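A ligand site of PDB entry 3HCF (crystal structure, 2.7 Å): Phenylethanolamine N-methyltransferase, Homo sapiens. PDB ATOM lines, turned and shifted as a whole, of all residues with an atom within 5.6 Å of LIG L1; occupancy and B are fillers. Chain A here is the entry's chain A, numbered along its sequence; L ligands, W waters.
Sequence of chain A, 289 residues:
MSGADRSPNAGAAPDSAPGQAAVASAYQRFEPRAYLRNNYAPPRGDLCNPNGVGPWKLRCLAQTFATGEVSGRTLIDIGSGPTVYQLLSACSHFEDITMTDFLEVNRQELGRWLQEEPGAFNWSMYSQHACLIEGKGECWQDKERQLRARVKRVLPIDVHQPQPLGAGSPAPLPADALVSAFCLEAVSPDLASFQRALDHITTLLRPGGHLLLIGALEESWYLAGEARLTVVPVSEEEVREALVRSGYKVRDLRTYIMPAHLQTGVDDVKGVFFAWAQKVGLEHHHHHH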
ATOM      1  N   TYR A  35     -29.320 -25.145   0.854  1.00  0.00           N
ATOM      2  CA  TYR A  35     -29.420 -26.003  -0.312  1.00  0.00           C
ATOM      3  C   TYR A  35     -30.871 -26.467  -0.498  1.00  0.00           C
ATOM      4  O   TYR A  35     -31.530 -26.114  -1.472  1.00  0.00           O
ATOM      5  CB  TYR A  35     -28.533 -27.226  -0.171  1.00  0.00           C
ATOM      6  CG  TYR A  35     -28.574 -28.143  -1.371  1.00  0.00           C
ATOM      7  CD1 TYR A  35     -28.216 -27.691  -2.628  1.00  0.00           C
ATOM      8  CD2 TYR A  35     -28.940 -29.480  -1.253  1.00  0.00           C
ATOM      9  CE1 TYR A  35     -28.240 -28.519  -3.734  1.00  0.00           C
ATOM     10  CE2 TYR A  35     -28.942 -30.314  -2.358  1.00  0.00           C
ATOM     11  CZ  TYR A  35     -28.601 -29.826  -3.589  1.00  0.00           C
ATOM     12  OH  TYR A  35     -28.591 -30.644  -4.683  1.00  0.00           O
ATOM     13  N   ASN A  39     -33.724 -25.661  -3.561  1.00  0.00           N
ATOM     14  CA  ASN A  39     -33.882 -26.690  -4.572  1.00  0.00           C
ATOM     15  C   ASN A  39     -34.954 -27.725  -4.323  1.00  0.00           C
ATOM     16  O   ASN A  39     -35.265 -28.531  -5.211  1.00  0.00           O
ATOM     17  CB  ASN A  39     -32.571 -27.415  -4.786  1.00  0.00           C
ATOM     18  CG  ASN A  39     -31.599 -26.570  -5.438  1.00  0.00           C
ATOM     19  OD1 ASN A  39     -31.872 -26.020  -6.500  1.00  0.00           O
ATOM     20  ND2 ASN A  39     -30.445 -26.427  -4.829  1.00  0.00           N
ATOM     21  N   TYR A  40     -35.509 -27.714  -3.113  1.00  0.00           N
ATOM     22  CA  TYR A  40     -36.538 -28.665  -2.755  1.00  0.00           C
ATOM     23  C   TYR A  40     -37.723 -28.014  -2.043  1.00  0.00           C
ATOM     24  O   TYR A  40     -38.636 -28.718  -1.633  1.00  0.00           O
ATOM     25  CB  TYR A  40     -35.932 -29.823  -1.960  1.00  0.00           C
ATOM     26  CG  TYR A  40     -34.888 -30.554  -2.799  1.00  0.00           C
ATOM     27  CD1 TYR A  40     -33.539 -30.196  -2.763  1.00  0.00           C
ATOM     28  CD2 TYR A  40     -35.270 -31.557  -3.666  1.00  0.00           C
ATOM     29  CE1 TYR A  40     -32.611 -30.872  -3.553  1.00  0.00           C
ATOM     30  CE2 TYR A  40     -34.349 -32.241  -4.446  1.00  0.00           C
ATOM     31  CZ  TYR A  40     -33.034 -31.900  -4.386  1.00  0.00           C
ATOM     32  OH  TYR A  40     -32.155 -32.581  -5.207  1.00  0.00           O
ATOM     33  N   ARG A  44     -39.464 -24.991  -6.961  1.00  0.00           N
ATOM     34  CA  ARG A  44     -38.982 -26.255  -7.504  1.00  0.00           C
ATOM     35  C   ARG A  44     -39.537 -27.369  -6.653  1.00  0.00           C
ATOM     36  O   ARG A  44     -39.726 -28.507  -7.146  1.00  0.00           O
ATOM     37  CB  ARG A  44     -37.441 -26.278  -7.528  1.00  0.00           C
ATOM     38  CG  ARG A  44     -36.825 -25.159  -8.380  1.00  0.00           C
ATOM     39  CD  ARG A  44     -35.300 -25.132  -8.292  1.00  0.00           C
ATOM     40  NE  ARG A  44     -34.701 -24.426  -9.419  1.00  0.00           N
ATOM     41  CZ  ARG A  44     -33.411 -24.481  -9.742  1.00  0.00           C
ATOM     42  NH1 ARG A  44     -32.549 -25.207  -9.021  1.00  0.00           N
ATOM     43  NH2 ARG A  44     -32.975 -23.810 -10.788  1.00  0.00           N
ATOM     44  N   VAL A  53     -39.698 -29.980 -12.211  1.00  0.00           N
ATOM     45  CA  VAL A  53     -38.513 -30.832 -12.276  1.00  0.00           C
ATOM     46  C   VAL A  53     -38.532 -31.972 -11.291  1.00  0.00           C
ATOM     47  O   VAL A  53     -37.966 -33.029 -11.566  1.00  0.00           O
ATOM     48  CB  VAL A  53     -37.157 -30.043 -12.074  1.00  0.00           C
ATOM     49  CG1 VAL A  53     -37.055 -29.428 -10.698  1.00  0.00           C
ATOM     50  CG2 VAL A  53     -35.949 -30.956 -12.346  1.00  0.00           C
ATOM     51  N   LYS A  57     -37.935 -35.884 -12.160  1.00  0.00           N
ATOM     52  CA  LYS A  57     -36.947 -36.750 -11.559  1.00  0.00           C
ATOM     53  C   LYS A  57     -37.669 -37.929 -10.969  1.00  0.00           C
ATOM     54  O   LYS A  57     -37.424 -39.055 -11.384  1.00  0.00           O
ATOM     55  CB  LYS A  57     -36.173 -36.032 -10.472  1.00  0.00           C
ATOM     56  CG  LYS A  57     -35.174 -35.010 -10.965  1.00  0.00           C
ATOM     57  CD  LYS A  57     -34.410 -34.410  -9.760  1.00  0.00           C
ATOM     58  CE  LYS A  57     -35.150 -33.245  -9.124  1.00  0.00           C
ATOM     59  NZ  LYS A  57     -34.446 -32.659  -7.953  1.00  0.00           N
ATOM     60  N   TYR A  85     -35.086 -38.124  -1.543  1.00  0.00           N
ATOM     61  CA  TYR A  85     -35.971 -38.384  -2.668  1.00  0.00           C
ATOM     62  C   TYR A  85     -35.349 -39.356  -3.650  1.00  0.00           C
ATOM     63  O   TYR A  85     -36.046 -40.182  -4.239  1.00  0.00           O
ATOM     64  CB  TYR A  85     -36.309 -37.092  -3.386  1.00  0.00           C
ATOM     65  CG  TYR A  85     -35.190 -36.567  -4.250  1.00  0.00           C
ATOM     66  CD1 TYR A  85     -35.178 -36.823  -5.592  1.00  0.00           C
ATOM     67  CD2 TYR A  85     -34.133 -35.838  -3.704  1.00  0.00           C
ATOM     68  CE1 TYR A  85     -34.156 -36.333  -6.400  1.00  0.00           C
ATOM     69  CE2 TYR A  85     -33.134 -35.342  -4.484  1.00  0.00           C
ATOM     70  CZ  TYR A  85     -33.134 -35.606  -5.831  1.00  0.00           C
ATOM     71  OH  TYR A  85     -32.116 -35.131  -6.623  1.00  0.00           O
ATOM     72  N   PHE A 182     -26.759 -35.117  -8.854  1.00  0.00           N
ATOM     73  CA  PHE A 182     -26.156 -33.779  -8.698  1.00  0.00           C
ATOM     74  C   PHE A 182     -24.834 -33.764  -7.885  1.00  0.00           C
ATOM     75  O   PHE A 182     -24.532 -32.787  -7.172  1.00  0.00           O
ATOM     76  CB  PHE A 182     -27.138 -32.799  -8.056  1.00  0.00           C
ATOM     77  CG  PHE A 182     -28.466 -32.712  -8.741  1.00  0.00           C
ATOM     78  CD1 PHE A 182     -29.600 -33.304  -8.192  1.00  0.00           C
ATOM     79  CD2 PHE A 182     -28.579 -32.002  -9.933  1.00  0.00           C
ATOM     80  CE1 PHE A 182     -30.801 -33.204  -8.823  1.00  0.00           C
ATOM     81  CE2 PHE A 182     -29.785 -31.888 -10.578  1.00  0.00           C
ATOM     82  CZ  PHE A 182     -30.894 -32.492 -10.019  1.00  0.00           C
ATOM     83  N   GLU A 185     -20.686 -34.099 -11.315  1.00  0.00           N
ATOM     84  CA  GLU A 185     -20.451 -32.869 -12.045  1.00  0.00           C
ATOM     85  C   GLU A 185     -20.356 -31.662 -11.100  1.00  0.00           C
ATOM     86  O   GLU A 185     -19.942 -30.585 -11.511  1.00  0.00           O
ATOM     87  CB  GLU A 185     -21.543 -32.664 -13.097  1.00  0.00           C
ATOM     88  CG  GLU A 185     -22.827 -32.083 -12.547  1.00  0.00           C
ATOM     89  CD  GLU A 185     -23.786 -33.144 -12.033  1.00  0.00           C
ATOM     90  OE1 GLU A 185     -23.480 -34.342 -12.197  1.00  0.00           O
ATOM     91  OE2 GLU A 185     -24.836 -32.776 -11.452  1.00  0.00           O
ATOM     92  N   ALA A 186     -20.739 -31.848  -9.851  1.00  0.00           N
ATOM     93  CA  ALA A 186     -20.680 -30.737  -8.914  1.00  0.00           C
ATOM     94  C   ALA A 186     -19.509 -30.817  -7.955  1.00  0.00           C
ATOM     95  O   ALA A 186     -19.327 -29.918  -7.134  1.00  0.00           O
ATOM     96  CB  ALA A 186     -21.962 -30.641  -8.157  1.00  0.00           C
ATOM     97  N   ALA A 216     -27.089 -32.194 -13.327  1.00  0.00           N
ATOM     98  CA  ALA A 216     -27.410 -30.949 -13.995  1.00  0.00           C
ATOM     99  C   ALA A 216     -26.734 -30.940 -15.369  1.00  0.00           C
ATOM    100  O   ALA A 216     -25.733 -31.628 -15.571  1.00  0.00           O
ATOM    101  CB  ALA A 216     -26.962 -29.791 -13.146  1.00  0.00           C
ATOM    102  N   GLU A 219     -24.653 -26.763 -16.303  1.00  0.00           N
ATOM    103  CA  GLU A 219     -24.651 -25.899 -15.111  1.00  0.00           C
ATOM    104  C   GLU A 219     -23.191 -25.558 -14.775  1.00  0.00           C
ATOM    105  O   GLU A 219     -22.298 -26.411 -14.925  1.00  0.00           O
ATOM    106  CB  GLU A 219     -25.275 -26.626 -13.926  1.00  0.00           C
ATOM    107  CG  GLU A 219     -25.256 -25.815 -12.649  1.00  0.00           C
ATOM    108  CD  GLU A 219     -25.522 -26.664 -11.404  1.00  0.00           C
ATOM    109  OE1 GLU A 219     -25.973 -26.123 -10.379  1.00  0.00           O
ATOM    110  OE2 GLU A 219     -25.300 -27.882 -11.457  1.00  0.00           O
ATOM    111  N   TYR A 222     -23.680 -22.910  -8.561  1.00  0.00           N
ATOM    112  CA  TYR A 222     -24.964 -22.914  -7.842  1.00  0.00           C
ATOM    113  C   TYR A 222     -24.724 -22.583  -6.385  1.00  0.00           C
ATOM    114  O   TYR A 222     -23.704 -22.993  -5.831  1.00  0.00           O
ATOM    115  CB  TYR A 222     -25.658 -24.266  -7.952  1.00  0.00           C
ATOM    116  CG  TYR A 222     -25.026 -25.315  -7.104  1.00  0.00           C
ATOM    117  CD1 TYR A 222     -25.237 -25.353  -5.746  1.00  0.00           C
ATOM    118  CD2 TYR A 222     -24.196 -26.277  -7.649  1.00  0.00           C
ATOM    119  CE1 TYR A 222     -24.660 -26.309  -4.961  1.00  0.00           C
ATOM    120  CE2 TYR A 222     -23.608 -27.239  -6.860  1.00  0.00           C
ATOM    121  CZ  TYR A 222     -23.837 -27.244  -5.521  1.00  0.00           C
ATOM    122  OH  TYR A 222     -23.274 -28.186  -4.704  1.00  0.00           O
ATOM    123  N   VAL A 231     -19.274 -25.669 -10.874  1.00  0.00           N
ATOM    124  CA  VAL A 231     -19.760 -26.881 -11.491  1.00  0.00           C
ATOM    125  C   VAL A 231     -19.146 -27.020 -12.871  1.00  0.00           C
ATOM    126  O   VAL A 231     -18.846 -26.016 -13.540  1.00  0.00           O
ATOM    127  CB  VAL A 231     -21.301 -26.812 -11.608  1.00  0.00           C
ATOM    128  CG1 VAL A 231     -21.921 -28.121 -12.215  1.00  0.00           C
ATOM    129  CG2 VAL A 231     -21.914 -26.503 -10.252  1.00  0.00           C
ATOM    130  N   MET A 258     -34.958 -27.108 -18.253  1.00  0.00           N
ATOM    131  CA  MET A 258     -35.485 -26.267 -17.187  1.00  0.00           C
ATOM    132  C   MET A 258     -36.422 -25.196 -17.768  1.00  0.00           C
ATOM    133  O   MET A 258     -36.091 -24.532 -18.743  1.00  0.00           O
ATOM    134  CB  MET A 258     -34.357 -25.659 -16.369  1.00  0.00           C
ATOM    135  CG  MET A 258     -34.737 -25.384 -14.925  1.00  0.00           C
ATOM    136  SD  MET A 258     -34.970 -26.832 -13.862  1.00  0.00           S
ATOM    137  CE  MET A 258     -33.369 -27.605 -13.937  1.00  0.00           C
ATOM    138  N   LEU A 262     -38.707 -22.000 -13.320  1.00  0.00           N
ATOM    139  CA  LEU A 262     -37.895 -22.724 -12.352  1.00  0.00           C
ATOM    140  C   LEU A 262     -36.443 -22.236 -12.357  1.00  0.00           C
ATOM    141  O   LEU A 262     -35.598 -22.779 -11.641  1.00  0.00           O
ATOM    142  CB  LEU A 262     -37.978 -24.209 -12.628  1.00  0.00           C
ATOM    143  CG  LEU A 262     -39.313 -24.815 -12.179  1.00  0.00           C
ATOM    144  CD1 LEU A 262     -39.337 -26.334 -12.322  1.00  0.00           C
ATOM    145  CD2 LEU A 262     -39.615 -24.427 -10.754  1.00  0.00           C
ATOM    146  N   VAL A 266     -30.519 -19.263  -8.042  1.00  0.00           N
ATOM    147  CA  VAL A 266     -29.694 -20.029  -7.119  1.00  0.00           C
ATOM    148  C   VAL A 266     -28.735 -20.797  -7.978  1.00  0.00           C
ATOM    149  O   VAL A 266     -27.936 -21.584  -7.479  1.00  0.00           O
ATOM    150  CB  VAL A 266     -30.525 -21.077  -6.310  1.00  0.00           C
ATOM    151  CG1 VAL A 266     -31.407 -20.376  -5.299  1.00  0.00           C
ATOM    152  CG2 VAL A 266     -31.321 -21.992  -7.264  1.00  0.00           C
ATOM    153  N   ASP A 267     -28.861 -20.638  -9.277  1.00  0.00           N
ATOM    154  CA  ASP A 267     -27.975 -21.328 -10.194  1.00  0.00           C
ATOM    155  C   ASP A 267     -28.201 -20.877 -11.622  1.00  0.00           C
ATOM    156  O   ASP A 267     -28.864 -19.850 -11.883  1.00  0.00           O
ATOM    157  CB  ASP A 267     -28.129 -22.817 -10.108  1.00  0.00           C
ATOM    158  CG  ASP A 267     -29.531 -23.220 -10.281  1.00  0.00           C
ATOM    159  OD1 ASP A 267     -30.161 -22.744 -11.306  1.00  0.00           O
ATOM    160  OD2 ASP A 267     -29.918 -24.004  -9.359  1.00  0.00           O
ATOM    161  N   VAL A 269     -28.156 -23.554 -14.085  1.00  0.00           N
ATOM    162  CA  VAL A 269     -28.524 -24.828 -14.744  1.00  0.00           C
ATOM    163  C   VAL A 269     -29.535 -24.632 -15.889  1.00  0.00           C
ATOM    164  O   VAL A 269     -30.427 -23.780 -15.812  1.00  0.00           O
ATOM    165  CB  VAL A 269     -29.097 -25.796 -13.720  1.00  0.00           C
ATOM    166  CG1 VAL A 269     -30.152 -25.068 -12.922  1.00  0.00           C
ATOM    167  CG2 VAL A 269     -29.651 -27.031 -14.406  1.00  0.00           C
ATOM    168  N   GLY A 271     -30.722 -27.541 -17.782  1.00  0.00           N
ATOM    169  CA  GLY A 271     -31.482 -28.765 -17.947  1.00  0.00           C
ATOM    170  C   GLY A 271     -31.048 -29.769 -16.889  1.00  0.00           C
ATOM    171  O   GLY A 271     -30.082 -29.504 -16.128  1.00  0.00           O
ATOM    172  N   VAL A 272     -31.769 -30.883 -16.792  1.00  0.00           N
ATOM    173  CA  VAL A 272     -31.386 -31.959 -15.871  1.00  0.00           C
ATOM    174  C   VAL A 272     -31.423 -33.235 -16.659  1.00  0.00           C
ATOM    175  O   VAL A 272     -32.283 -33.387 -17.534  1.00  0.00           O
ATOM    176  CB  VAL A 272     -32.350 -32.114 -14.693  1.00  0.00           C
ATOM    177  CG1 VAL A 272     -32.075 -33.404 -13.938  1.00  0.00           C
ATOM    178  CG2 VAL A 272     -32.314 -30.892 -13.771  1.00  0.00           C
HETATM  179  F1  LIG L   1     -32.766 -29.204 -11.598  1.00  0.00           F
HETATM  180  C1  LIG L   1     -32.593 -28.218 -10.662  1.00  0.00           C
HETATM  181  F2  LIG L   1     -33.796 -27.788 -10.168  1.00  0.00           F
HETATM  182  F3  LIG L   1     -31.981 -27.141 -11.226  1.00  0.00           F
HETATM  183  C2  LIG L   1     -31.679 -28.686  -9.543  1.00  0.00           C
HETATM  184  C3  LIG L   1     -30.443 -28.097  -9.505  1.00  0.00           C
HETATM  185  C4  LIG L   1     -32.024 -29.629  -8.587  1.00  0.00           C
HETATM  186  C5  LIG L   1     -31.105 -29.952  -7.601  1.00  0.00           C
HETATM  187  C6  LIG L   1     -29.833 -29.358  -7.543  1.00  0.00           C
HETATM  188  C7  LIG L   1     -29.505 -28.418  -8.524  1.00  0.00           C
HETATM  189  C8  LIG L   1     -28.202 -27.611  -8.558  1.00  0.00           C
HETATM  190  O1  LIG L   1     -28.457 -26.313  -8.046  1.00  0.00           O
HETATM  191  C9  LIG L   1     -27.079 -28.348  -7.794  1.00  0.00           C
HETATM  192  N1  LIG L   1     -26.349 -29.250  -8.660  1.00  0.00           N
HETATM  193  N1  LG2 L   2     -27.772 -35.859  -4.095  1.00  0.00           N
HETATM  194  C1  LG2 L   2     -28.351 -34.626  -3.577  1.00  0.00           C
HETATM  195  C2  LG2 L   2     -27.357 -33.550  -3.121  1.00  0.00           C
HETATM  196  C3  LG2 L   2     -26.284 -33.197  -4.176  1.00  0.00           C
HETATM  197  S1  LG2 L   2     -25.261 -31.750  -3.732  1.00  0.00           S
HETATM  198  C4  LG2 L   2     -29.331 -34.010  -4.547  1.00  0.00           C
HETATM  199  O1  LG2 L   2     -29.626 -32.901  -4.286  1.00  0.00           O
HETATM  200  O2  LG2 L   2     -29.932 -34.851  -5.483  1.00  0.00           O
HETATM  201  C5  LG2 L   2     -23.565 -32.368  -3.948  1.00  0.00           C
HETATM  202  C6  LG2 L   2     -23.005 -33.166  -2.779  1.00  0.00           C
HETATM  203  O3  LG2 L   2     -21.740 -33.613  -3.083  1.00  0.00           O
HETATM  204  C7  LG2 L   2     -22.860 -32.337  -1.528  1.00  0.00           C
HETATM  205  O4  LG2 L   2     -23.638 -32.884  -0.517  1.00  0.00           O
HETATM  206  C8  LG2 L   2     -21.533 -32.427  -1.201  1.00  0.00           C
HETATM  207  O5  LG2 L   2     -21.290 -32.439   0.155  1.00  0.00           O
HETATM  208  C9  LG2 L   2     -21.056 -33.575  -1.887  1.00  0.00           C
HETATM  209  N2  LG2 L   2     -19.620 -33.614  -2.117  1.00  0.00           N
HETATM  210  C10 LG2 L   2     -18.755 -32.590  -2.092  1.00  0.00           C
HETATM  211  N3  LG2 L   2     -17.498 -33.066  -2.393  1.00  0.00           N
HETATM  212  C11 LG2 L   2     -17.598 -34.410  -2.613  1.00  0.00           C
HETATM  213  C12 LG2 L   2     -16.672 -35.372  -2.949  1.00  0.00           C
HETATM  214  N4  LG2 L   2     -15.287 -34.967  -3.152  1.00  0.00           N
HETATM  215  N5  LG2 L   2     -17.062 -36.640  -3.098  1.00  0.00           N
HETATM  216  C13 LG2 L   2     -18.356 -36.980  -2.922  1.00  0.00           C
HETATM  217  N6  LG2 L   2     -19.280 -36.046  -2.585  1.00  0.00           N
HETATM  218  C14 LG2 L   2     -18.892 -34.764  -2.436  1.00  0.00           C
HETATM  219  O   HOH W   1     -29.042 -24.334  -5.693  1.00  0.00           O
HETATM  220  O   HOH W   2     -24.636 -30.322 -10.181  1.00  0.00           O
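NH1 of Arg 44 is in salt-bridge range of OD2 of Asp 267 (2.9 Å). NH1 of Arg 44 lies within hydrogen-bond range of OD1 of Asn 39, 2.7 Å away. The backbone carbonyl oxygen (O) of Leu 262 sits at hydrogen-bond distance from the guanidinium group (NE) of Arg 44 (2.9 Å). OH of Tyr 40 is in hydrogen-bond range of OH of Tyr 85, 2.9 Å away.
A fluorine (F3) of LIG L1 sits close to the guanidinium group (NH1) of Arg 44, 3.0 Å away. Tyr 35 touches LIG L1. Asn 39 touches LIG L1. OH of Tyr 40 touches C5 of LIG L1, at 3.7 Å. CG1 of Val 53 touches F2 of LIG L1 (3.7 Å). NZ of Lys 57 touches C4 of LIG L1 (3.9 Å). CZ of Phe 182 touches C4 of LIG L1, at 3.4 Å. Tyr 222 touches LIG L1 (CB to O1, 3.5 Å). CE of Met 258 touches F1 of LIG L1, at 2.9 Å. CG1 of Val 269 touches F3 of LIG L1, 3.2 Å away. Val 272 touches LIG L1.
Water W2 lies within hydrogen-bond range of N1 of LIG L1 (2.5 Å), OE2 of Glu 185 (2.8 Å) and OE2 of Glu 219 (2.8 Å). Water W1 lies within hydrogen-bond range of ND2 of Asn 39 (2.7 Å), O1 of LIG L1 (3.1 Å) and O of Val 266 (3.5 Å).
An oxygen (O1) of LIG L1 lies within hydrogen-bond range of the side-chain carboxylate (OD2) of Asp 267 (3.0 Å). The side-chain carboxylate (OE2) of Glu 219 lies within salt-bridge range of a nitrogen (N1) of LIG L1 (3.3 Å). An oxygen (O1) of LG2 L2 lies within hydrogen-bond range of the side-chain hydroxyl (OH) of Tyr 35, at 2.5 Å. The side-chain hydroxyl of Tyr 40 lies within hydrogen-bond range of an oxygen (O1) of LG2 L2, 2.7 Å away. O2 of LG2 L2 sits at hydrogen-bond distance from OH of Tyr 85 (2.5 Å).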
